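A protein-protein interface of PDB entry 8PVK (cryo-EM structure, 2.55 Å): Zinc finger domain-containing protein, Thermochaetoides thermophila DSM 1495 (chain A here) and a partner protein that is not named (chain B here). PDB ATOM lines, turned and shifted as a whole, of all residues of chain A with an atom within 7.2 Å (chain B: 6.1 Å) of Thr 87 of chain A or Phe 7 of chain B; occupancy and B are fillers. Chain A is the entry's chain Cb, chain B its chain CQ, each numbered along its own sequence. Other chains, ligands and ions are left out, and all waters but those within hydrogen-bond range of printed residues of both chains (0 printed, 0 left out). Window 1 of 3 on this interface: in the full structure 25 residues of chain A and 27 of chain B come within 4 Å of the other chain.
The backbone carbonyl oxygen of Phe 7 of chain B lies close to the side-chain hydroxyl of Tyr 86 of chain A (3.3 Å). NE2 of His 88 of chain A sits at hydrogen-bond distance from O of Ala 28 of chain B, at 3.1 Å. NH2 of Arg 47 of chain B lies within hydrogen-bond range of O of Gly 84 of chain A (2.9 Å). The guanidinium group (NE) of Arg 47 of chain B lies within salt-bridge range of the side-chain carboxylate (OE2) of Glu 90 of chain A (2.6 Å).
The backbone carbonyl oxygen (O) of Arg 30 of chain B sits at hydrogen-bond distance from the backbone NH (N) of Phe 7 of chain B (2.8 Å). OE2 of Glu 23 of chain A lies within hydrogen-bond range of N of Ala 85 of chain A. The side-chain carboxylate (OE1) of Glu 89 of chain A sits close to the side-chain hydroxyl (OG1) of Thr 87 of chain A, at 3.4 Å.
Ala 85 of chain A touches Arg 47 of chain B. CG of Pro 46 of chain B touches CD1 of Tyr 86 of chain A, at 3.7 Å. Thr 87 of chain A touches Phe 7 of chain B. Phe 7 of chain B touches His 88 of chain A (CD1 to NE2, 3.6 Å). Phe 29 of chain B touches His 88 of chain A (CE2 to CE1, 3.5 Å). CB of Ala 91 of chain A touches O of Phe 7 of chain B, 3.96 Å away.
Of chain A, only Tyr 86, Thr 87, His 88 and Ala 91 come within 4 Å of Phe 7 of chain B. Of the printed residues of chain A, Ala 28 of chain B touches His 88. Printed residues of chain B within 4 Å of Tyr 86 of chain A: Phe 7 and Pro 46. Of the printed residues of chain B, His 88 of chain A touches Phe 7, Ala 28 and Phe 29. Of the printed residues of chain B, Ala 85 of chain A touches Arg 47. Cys 9 of chain B touches none of the printed residues of chain A. Glu 89 of chain A touches none of the printed residues of chain B. The nearest residue of chain A that does not touch Phe 7 of chain B is Asp 20 of chain A (5.7 Å).
Printed residues of chain A that touch a printed residue of chain B: Gly 84, Ala 85, Tyr 86, Thr 87, His 88, Glu 90 and Ala 91. Hydrophobic or aromatic side chains of chain A within 4 Å of the printed part of chain B: Tyr 86, His 88 and Ala 91. Along chain A the printed residues that touch a printed residue of chain B span positions 84 to 91. Of the 14 printed residues of chain B, 5 touch a printed residue of chain A. Printed residues of chain B that touch a printed residue of chain A: Phe 7, Ala 28, Phe 29, Pro 46 and Arg 47. Hydrophobic or aromatic side chains of chain B within 4 Å of the printed part of chain A: Phe 7, Phe 29 and Pro 46.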
ATOM      1  N   ASP A  20      -8.073   6.051  25.294  1.00  0.00           N
ATOM      2  CA  ASP A  20      -8.513   4.692  24.988  1.00  0.00           C
ATOM      3  C   ASP A  20      -9.479   4.169  26.044  1.00  0.00           C
ATOM      4  O   ASP A  20     -10.423   3.436  25.716  1.00  0.00           O
ATOM      5  CB  ASP A  20      -7.309   3.760  24.846  1.00  0.00           C
ATOM      6  CG  ASP A  20      -6.349   3.857  26.013  1.00  0.00           C
ATOM      7  OD1 ASP A  20      -6.586   4.682  26.915  1.00  0.00           O
ATOM      8  OD2 ASP A  20      -5.352   3.105  26.026  1.00  0.00           O
ATOM      9  N   GLU A  23     -12.692   5.693  25.065  1.00  0.00           N
ATOM     10  CA  GLU A  23     -13.304   4.942  23.965  1.00  0.00           C
ATOM     11  C   GLU A  23     -13.964   3.659  24.452  1.00  0.00           C
ATOM     12  O   GLU A  23     -15.069   3.320  24.013  1.00  0.00           O
ATOM     13  CB  GLU A  23     -12.285   4.599  22.878  1.00  0.00           C
ATOM     14  CG  GLU A  23     -11.738   5.758  22.095  1.00  0.00           C
ATOM     15  CD  GLU A  23     -10.734   5.311  21.054  1.00  0.00           C
ATOM     16  OE1 GLU A  23     -10.383   4.114  21.043  1.00  0.00           O
ATOM     17  OE2 GLU A  23     -10.334   6.145  20.216  1.00  0.00           O
ATOM     18  N   ARG A  24     -13.295   2.921  25.341  1.00  0.00           N
ATOM     19  CA  ARG A  24     -13.906   1.712  25.887  1.00  0.00           C
ATOM     20  C   ARG A  24     -15.102   2.035  26.778  1.00  0.00           C
ATOM     21  O   ARG A  24     -16.039   1.234  26.864  1.00  0.00           O
ATOM     22  CB  ARG A  24     -12.870   0.888  26.652  1.00  0.00           C
ATOM     23  CG  ARG A  24     -12.139  -0.134  25.792  1.00  0.00           C
ATOM     24  CD  ARG A  24     -11.360  -1.135  26.646  1.00  0.00           C
ATOM     25  NE  ARG A  24     -10.319  -0.519  27.464  1.00  0.00           N
ATOM     26  CZ  ARG A  24      -9.196   0.015  27.001  1.00  0.00           C
ATOM     27  NH1 ARG A  24      -8.883  -0.029  25.715  1.00  0.00           N
ATOM     28  NH2 ARG A  24      -8.350   0.586  27.853  1.00  0.00           N
ATOM     29  N   ARG A  27     -17.876   2.652  24.250  1.00  0.00           N
ATOM     30  CA  ARG A  27     -18.295   1.440  23.557  1.00  0.00           C
ATOM     31  C   ARG A  27     -19.006   0.464  24.486  1.00  0.00           C
ATOM     32  O   ARG A  27     -19.966  -0.197  24.073  1.00  0.00           O
ATOM     33  CB  ARG A  27     -17.085   0.765  22.909  1.00  0.00           C
ATOM     34  CG  ARG A  27     -17.426  -0.072  21.684  1.00  0.00           C
ATOM     35  CD  ARG A  27     -16.302  -1.008  21.191  1.00  0.00           C
ATOM     36  NE  ARG A  27     -14.959  -0.431  21.147  1.00  0.00           N
ATOM     37  CZ  ARG A  27     -14.064  -0.506  22.124  1.00  0.00           C
ATOM     38  NH1 ARG A  27     -14.322  -1.149  23.252  1.00  0.00           N
ATOM     39  NH2 ARG A  27     -12.876   0.071  21.961  1.00  0.00           N
ATOM     40  N   GLY A  84      -9.324   8.631  16.720  1.00  0.00           N
ATOM     41  CA  GLY A  84      -9.054   7.341  17.326  1.00  0.00           C
ATOM     42  C   GLY A  84      -7.844   7.366  18.234  1.00  0.00           C
ATOM     43  O   GLY A  84      -6.789   7.881  17.853  1.00  0.00           O
ATOM     44  N   ALA A  85      -7.981   6.813  19.435  1.00  0.00           N
ATOM     45  CA  ALA A  85      -6.897   6.821  20.406  1.00  0.00           C
ATOM     46  C   ALA A  85      -5.824   5.807  20.040  1.00  0.00           C
ATOM     47  O   ALA A  85      -6.066   4.846  19.304  1.00  0.00           O
ATOM     48  CB  ALA A  85      -7.420   6.522  21.809  1.00  0.00           C
ATOM     49  N   TYR A  86      -4.628   6.032  20.573  1.00  0.00           N
ATOM     50  CA  TYR A  86      -3.506   5.129  20.363  1.00  0.00           C
ATOM     51  C   TYR A  86      -3.623   3.919  21.280  1.00  0.00           C
ATOM     52  O   TYR A  86      -3.897   4.059  22.476  1.00  0.00           O
ATOM     53  CB  TYR A  86      -2.192   5.865  20.615  1.00  0.00           C
ATOM     54  CG  TYR A  86      -0.971   5.166  20.076  1.00  0.00           C
ATOM     55  CD1 TYR A  86      -0.008   4.660  20.935  1.00  0.00           C
ATOM     56  CD2 TYR A  86      -0.780   5.009  18.712  1.00  0.00           C
ATOM     57  CE1 TYR A  86       1.112   4.023  20.452  1.00  0.00           C
ATOM     58  CE2 TYR A  86       0.333   4.369  18.223  1.00  0.00           C
ATOM     59  CZ  TYR A  86       1.279   3.881  19.095  1.00  0.00           C
ATOM     60  OH  TYR A  86       2.394   3.246  18.603  1.00  0.00           O
ATOM     61  N   THR A  87      -3.413   2.732  20.716  1.00  0.00           N
ATOM     62  CA  THR A  87      -3.549   1.477  21.439  1.00  0.00           C
ATOM     63  C   THR A  87      -2.338   0.586  21.188  1.00  0.00           C
ATOM     64  O   THR A  87      -1.475   0.876  20.353  1.00  0.00           O
ATOM     65  CB  THR A  87      -4.830   0.728  21.036  1.00  0.00           C
ATOM     66  OG1 THR A  87      -4.894   0.620  19.609  1.00  0.00           O
ATOM     67  CG2 THR A  87      -6.075   1.440  21.552  1.00  0.00           C
ATOM     68  N   HIS A  88      -2.302  -0.530  21.926  1.00  0.00           N
ATOM     69  CA  HIS A  88      -1.240  -1.517  21.754  1.00  0.00           C
ATOM     70  C   HIS A  88      -1.337  -2.225  20.410  1.00  0.00           C
ATOM     71  O   HIS A  88      -0.309  -2.628  19.853  1.00  0.00           O
ATOM     72  CB  HIS A  88      -1.281  -2.542  22.886  1.00  0.00           C
ATOM     73  CG  HIS A  88      -0.554  -2.109  24.121  1.00  0.00           C
ATOM     74  ND1 HIS A  88      -1.191  -1.515  25.188  1.00  0.00           N
ATOM     75  CD2 HIS A  88       0.753  -2.191  24.461  1.00  0.00           C
ATOM     76  CE1 HIS A  88      -0.307  -1.244  26.131  1.00  0.00           C
ATOM     77  NE2 HIS A  88       0.881  -1.645  25.714  1.00  0.00           N
ATOM     78  N   GLU A  89      -2.552  -2.395  19.881  1.00  0.00           N
ATOM     79  CA  GLU A  89      -2.713  -2.986  18.555  1.00  0.00           C
ATOM     80  C   GLU A  89      -2.093  -2.100  17.479  1.00  0.00           C
ATOM     81  O   GLU A  89      -1.381  -2.586  16.592  1.00  0.00           O
ATOM     82  CB  GLU A  89      -4.195  -3.237  18.264  1.00  0.00           C
ATOM     83  CG  GLU A  89      -4.851  -4.311  19.130  1.00  0.00           C
ATOM     84  CD  GLU A  89      -5.301  -3.807  20.489  1.00  0.00           C
ATOM     85  OE1 GLU A  89      -5.168  -2.595  20.758  1.00  0.00           O
ATOM     86  OE2 GLU A  89      -5.793  -4.629  21.290  1.00  0.00           O
ATOM     87  N   GLU A  90      -2.337  -0.790  17.559  1.00  0.00           N
ATOM     88  CA  GLU A  90      -1.706   0.134  16.624  1.00  0.00           C
ATOM     89  C   GLU A  90      -0.200   0.210  16.855  1.00  0.00           C
ATOM     90  O   GLU A  90       0.566   0.366  15.895  1.00  0.00           O
ATOM     91  CB  GLU A  90      -2.356   1.516  16.738  1.00  0.00           C
ATOM     92  CG  GLU A  90      -1.705   2.606  15.899  1.00  0.00           C
ATOM     93  CD  GLU A  90      -2.491   3.900  15.901  1.00  0.00           C
ATOM     94  OE1 GLU A  90      -3.449   4.015  16.693  1.00  0.00           O
ATOM     95  OE2 GLU A  90      -2.146   4.805  15.113  1.00  0.00           O
ATOM     96  N   ALA A  91       0.241   0.066  18.109  1.00  0.00           N
ATOM     97  CA  ALA A  91       1.673   0.031  18.398  1.00  0.00           C
ATOM     98  C   ALA A  91       2.349  -1.177  17.753  1.00  0.00           C
ATOM     99  O   ALA A  91       3.467  -1.066  17.235  1.00  0.00           O
ATOM    100  CB  ALA A  91       1.901   0.033  19.909  1.00  0.00           C
ATOM    101  N   MET A  92       1.694  -2.340  17.785  1.00  0.00           N
ATOM    102  CA  MET A  92       2.241  -3.516  17.111  1.00  0.00           C
ATOM    103  C   MET A  92       2.195  -3.363  15.594  1.00  0.00           C
ATOM    104  O   MET A  92       3.137  -3.761  14.896  1.00  0.00           O
ATOM    105  CB  MET A  92       1.492  -4.779  17.536  1.00  0.00           C
ATOM    106  CG  MET A  92       1.678  -5.165  18.988  1.00  0.00           C
ATOM    107  SD  MET A  92       0.818  -6.697  19.388  1.00  0.00           S
ATOM    108  CE  MET A  92      -0.879  -6.133  19.419  1.00  0.00           C
ATOM    109  N   ALA A  93       1.105  -2.799  15.066  1.00  0.00           N
ATOM    110  CA  ALA A  93       0.992  -2.606  13.625  1.00  0.00           C
ATOM    111  C   ALA A  93       1.979  -1.575  13.094  1.00  0.00           C
ATOM    112  O   ALA A  93       2.312  -1.610  11.905  1.00  0.00           O
ATOM    113  CB  ALA A  93      -0.434  -2.197  13.260  1.00  0.00           C
ATOM    114  N   ALA A  94       2.447  -0.659  13.946  1.00  0.00           N
ATOM    115  CA  ALA A  94       3.447   0.315  13.524  1.00  0.00           C
ATOM    116  C   ALA A  94       4.785  -0.341  13.216  1.00  0.00           C
ATOM    117  O   ALA A  94       5.510   0.120  12.326  1.00  0.00           O
ATOM    118  CB  ALA A  94       3.621   1.386  14.600  1.00  0.00           C
ATOM    119  N   ASN B   5       9.412  -3.689  22.704  1.00  0.00           N
ATOM    120  CA  ASN B   5       9.370  -2.494  21.878  1.00  0.00           C
ATOM    121  C   ASN B   5       8.688  -1.386  22.659  1.00  0.00           C
ATOM    122  O   ASN B   5       7.782  -1.647  23.456  1.00  0.00           O
ATOM    123  CB  ASN B   5       8.645  -2.750  20.556  1.00  0.00           C
ATOM    124  CG  ASN B   5       9.555  -3.360  19.507  1.00  0.00           C
ATOM    125  OD1 ASN B   5      10.095  -2.659  18.652  1.00  0.00           O
ATOM    126  ND2 ASN B   5       9.732  -4.673  19.571  1.00  0.00           N
ATOM    127  N   CYS B   6       9.149  -0.156  22.446  1.00  0.00           N
ATOM    128  CA  CYS B   6       8.564   0.990  23.125  1.00  0.00           C
ATOM    129  C   CYS B   6       7.130   1.191  22.659  1.00  0.00           C
ATOM    130  O   CYS B   6       6.836   1.091  21.465  1.00  0.00           O
ATOM    131  CB  CYS B   6       9.391   2.246  22.860  1.00  0.00           C
ATOM    132  SG  CYS B   6       8.691   3.756  23.564  1.00  0.00           S
ATOM    133  N   PHE B   7       6.236   1.448  23.613  1.00  0.00           N
ATOM    134  CA  PHE B   7       4.841   1.698  23.274  1.00  0.00           C
ATOM    135  C   PHE B   7       4.698   2.981  22.466  1.00  0.00           C
ATOM    136  O   PHE B   7       3.880   3.054  21.544  1.00  0.00           O
ATOM    137  CB  PHE B   7       4.001   1.762  24.551  1.00  0.00           C
ATOM    138  CG  PHE B   7       2.568   2.149  24.323  1.00  0.00           C
ATOM    139  CD1 PHE B   7       1.670   1.242  23.786  1.00  0.00           C
ATOM    140  CD2 PHE B   7       2.117   3.417  24.657  1.00  0.00           C
ATOM    141  CE1 PHE B   7       0.350   1.592  23.578  1.00  0.00           C
ATOM    142  CE2 PHE B   7       0.797   3.773  24.453  1.00  0.00           C
ATOM    143  CZ  PHE B   7      -0.087   2.858  23.914  1.00  0.00           C
ATOM    144  N   PHE B   8       5.508   3.990  22.780  1.00  0.00           N
ATOM    145  CA  PHE B   8       5.328   5.304  22.178  1.00  0.00           C
ATOM    146  C   PHE B   8       5.987   5.400  20.805  1.00  0.00           C
ATOM    147  O   PHE B   8       5.347   5.811  19.832  1.00  0.00           O
ATOM    148  CB  PHE B   8       5.878   6.379  23.115  1.00  0.00           C
ATOM    149  CG  PHE B   8       5.196   7.704  22.979  1.00  0.00           C
ATOM    150  CD1 PHE B   8       5.651   8.643  22.070  1.00  0.00           C
ATOM    151  CD2 PHE B   8       4.094   8.009  23.759  1.00  0.00           C
ATOM    152  CE1 PHE B   8       5.021   9.861  21.945  1.00  0.00           C
ATOM    153  CE2 PHE B   8       3.460   9.228  23.638  1.00  0.00           C
ATOM    154  CZ  PHE B   8       3.922  10.153  22.727  1.00  0.00           C
ATOM    155  N   CYS B   9       7.262   5.026  20.702  1.00  0.00           N
ATOM    156  CA  CYS B   9       8.023   5.248  19.481  1.00  0.00           C
ATOM    157  C   CYS B   9       8.451   3.973  18.768  1.00  0.00           C
ATOM    158  O   CYS B   9       8.968   4.059  17.650  1.00  0.00           O
ATOM    159  CB  CYS B   9       9.267   6.093  19.784  1.00  0.00           C
ATOM    160  SG  CYS B   9      10.589   5.182  20.593  1.00  0.00           S
ATOM    161  N   GLY B  10       8.268   2.805  19.376  1.00  0.00           N
ATOM    162  CA  GLY B  10       8.576   1.559  18.705  1.00  0.00           C
ATOM    163  C   GLY B  10      10.039   1.180  18.652  1.00  0.00           C
ATOM    164  O   GLY B  10      10.377   0.191  17.991  1.00  0.00           O
ATOM    165  N   ALA B  28      -0.041  -2.683  30.918  1.00  0.00           N
ATOM    166  CA  ALA B  28       1.329  -2.234  31.106  1.00  0.00           C
ATOM    167  C   ALA B  28       1.810  -1.500  29.861  1.00  0.00           C
ATOM    168  O   ALA B  28       1.577  -1.935  28.731  1.00  0.00           O
ATOM    169  CB  ALA B  28       2.255  -3.413  31.412  1.00  0.00           C
ATOM    170  N   PHE B  29       2.484  -0.374  30.080  1.00  0.00           N
ATOM    171  CA  PHE B  29       2.998   0.460  29.002  1.00  0.00           C
ATOM    172  C   PHE B  29       4.503   0.581  29.172  1.00  0.00           C
ATOM    173  O   PHE B  29       4.968   1.190  30.137  1.00  0.00           O
ATOM    174  CB  PHE B  29       2.351   1.847  29.017  1.00  0.00           C
ATOM    175  CG  PHE B  29       0.871   1.832  28.776  1.00  0.00           C
ATOM    176  CD1 PHE B  29      -0.015   1.698  29.832  1.00  0.00           C
ATOM    177  CD2 PHE B  29       0.364   1.959  27.495  1.00  0.00           C
ATOM    178  CE1 PHE B  29      -1.379   1.685  29.614  1.00  0.00           C
ATOM    179  CE2 PHE B  29      -0.999   1.948  27.269  1.00  0.00           C
ATOM    180  CZ  PHE B  29      -1.870   1.809  28.330  1.00  0.00           C
ATOM    181  N   ARG B  30       5.258   0.020  28.236  1.00  0.00           N
ATOM    182  CA  ARG B  30       6.712   0.013  28.312  1.00  0.00           C
ATOM    183  C   ARG B  30       7.273   1.138  27.453  1.00  0.00           C
ATOM    184  O   ARG B  30       6.963   1.229  26.262  1.00  0.00           O
ATOM    185  CB  ARG B  30       7.275  -1.334  27.859  1.00  0.00           C
ATOM    186  CG  ARG B  30       8.789  -1.368  27.754  1.00  0.00           C
ATOM    187  CD  ARG B  30       9.439  -1.359  29.127  1.00  0.00           C
ATOM    188  NE  ARG B  30      10.888  -1.233  29.043  1.00  0.00           N
ATOM    189  CZ  ARG B  30      11.723  -2.247  28.867  1.00  0.00           C
ATOM    190  NH1 ARG B  30      11.285  -3.490  28.760  1.00  0.00           N
ATOM    191  NH2 ARG B  30      13.028  -2.009  28.794  1.00  0.00           N
ATOM    192  N   PHE B  31       8.094   1.991  28.059  1.00  0.00           N
ATOM    193  CA  PHE B  31       8.733   3.103  27.376  1.00  0.00           C
ATOM    194  C   PHE B  31      10.236   2.907  27.429  1.00  0.00           C
ATOM    195  O   PHE B  31      10.789   2.578  28.483  1.00  0.00           O
ATOM    196  CB  PHE B  31       8.362   4.440  28.018  1.00  0.00           C
ATOM    197  CG  PHE B  31       6.891   4.632  28.191  1.00  0.00           C
ATOM    198  CD1 PHE B  31       6.099   5.005  27.119  1.00  0.00           C
ATOM    199  CD2 PHE B  31       6.295   4.424  29.423  1.00  0.00           C
ATOM    200  CE1 PHE B  31       4.742   5.172  27.276  1.00  0.00           C
ATOM    201  CE2 PHE B  31       4.939   4.589  29.585  1.00  0.00           C
ATOM    202  CZ  PHE B  31       4.161   4.961  28.511  1.00  0.00           C
ATOM    203  N   CYS B  32      10.890   3.116  26.287  1.00  0.00           N
ATOM    204  CA  CYS B  32      12.330   2.924  26.206  1.00  0.00           C
ATOM    205  C   CYS B  32      13.111   4.048  26.874  1.00  0.00           C
ATOM    206  O   CYS B  32      14.285   3.851  27.202  1.00  0.00           O
ATOM    207  CB  CYS B  32      12.756   2.788  24.743  1.00  0.00           C
ATOM    208  SG  CYS B  32      12.460   4.261  23.732  1.00  0.00           S
ATOM    209  N   PHE B  40       4.129  10.697  26.959  1.00  0.00           N
ATOM    210  CA  PHE B  40       2.941   9.955  27.374  1.00  0.00           C
ATOM    211  C   PHE B  40       2.253  10.617  28.565  1.00  0.00           C
ATOM    212  O   PHE B  40       1.020  10.681  28.620  1.00  0.00           O
ATOM    213  CB  PHE B  40       3.326   8.512  27.702  1.00  0.00           C
ATOM    214  CG  PHE B  40       2.167   7.641  28.094  1.00  0.00           C
ATOM    215  CD1 PHE B  40       1.400   7.012  27.128  1.00  0.00           C
ATOM    216  CD2 PHE B  40       1.866   7.420  29.431  1.00  0.00           C
ATOM    217  CE1 PHE B  40       0.341   6.202  27.487  1.00  0.00           C
ATOM    218  CE2 PHE B  40       0.809   6.615  29.794  1.00  0.00           C
ATOM    219  CZ  PHE B  40       0.046   6.003  28.821  1.00  0.00           C
ATOM    220  N   PRO B  46       1.418   9.717  19.698  1.00  0.00           N
ATOM    221  CA  PRO B  46       2.536   9.208  18.884  1.00  0.00           C
ATOM    222  C   PRO B  46       2.256   9.226  17.393  1.00  0.00           C
ATOM    223  O   PRO B  46       3.187   9.403  16.598  1.00  0.00           O
ATOM    224  CB  PRO B  46       2.724   7.773  19.398  1.00  0.00           C
ATOM    225  CG  PRO B  46       2.058   7.738  20.725  1.00  0.00           C
ATOM    226  CD  PRO B  46       0.938   8.721  20.669  1.00  0.00           C
ATOM    227  N   ARG B  47       0.996   9.040  16.994  1.00  0.00           N
ATOM    228  CA  ARG B  47       0.619   9.128  15.590  1.00  0.00           C
ATOM    229  C   ARG B  47       0.804  10.531  15.029  1.00  0.00           C
ATOM    230  O   ARG B  47       0.978  10.683  13.816  1.00  0.00           O
ATOM    231  CB  ARG B  47      -0.832   8.677  15.421  1.00  0.00           C
ATOM    232  CG  ARG B  47      -1.208   8.239  14.019  1.00  0.00           C
ATOM    233  CD  ARG B  47      -2.716   8.137  13.879  1.00  0.00           C
ATOM    234  NE  ARG B  47      -3.280   7.178  14.820  1.00  0.00           N
ATOM    235  CZ  ARG B  47      -4.203   7.472  15.726  1.00  0.00           C
ATOM    236  NH1 ARG B  47      -4.696   8.693  15.841  1.00  0.00           N
ATOM    237  NH2 ARG B  47      -4.640   6.514  16.539  1.00  0.00           N
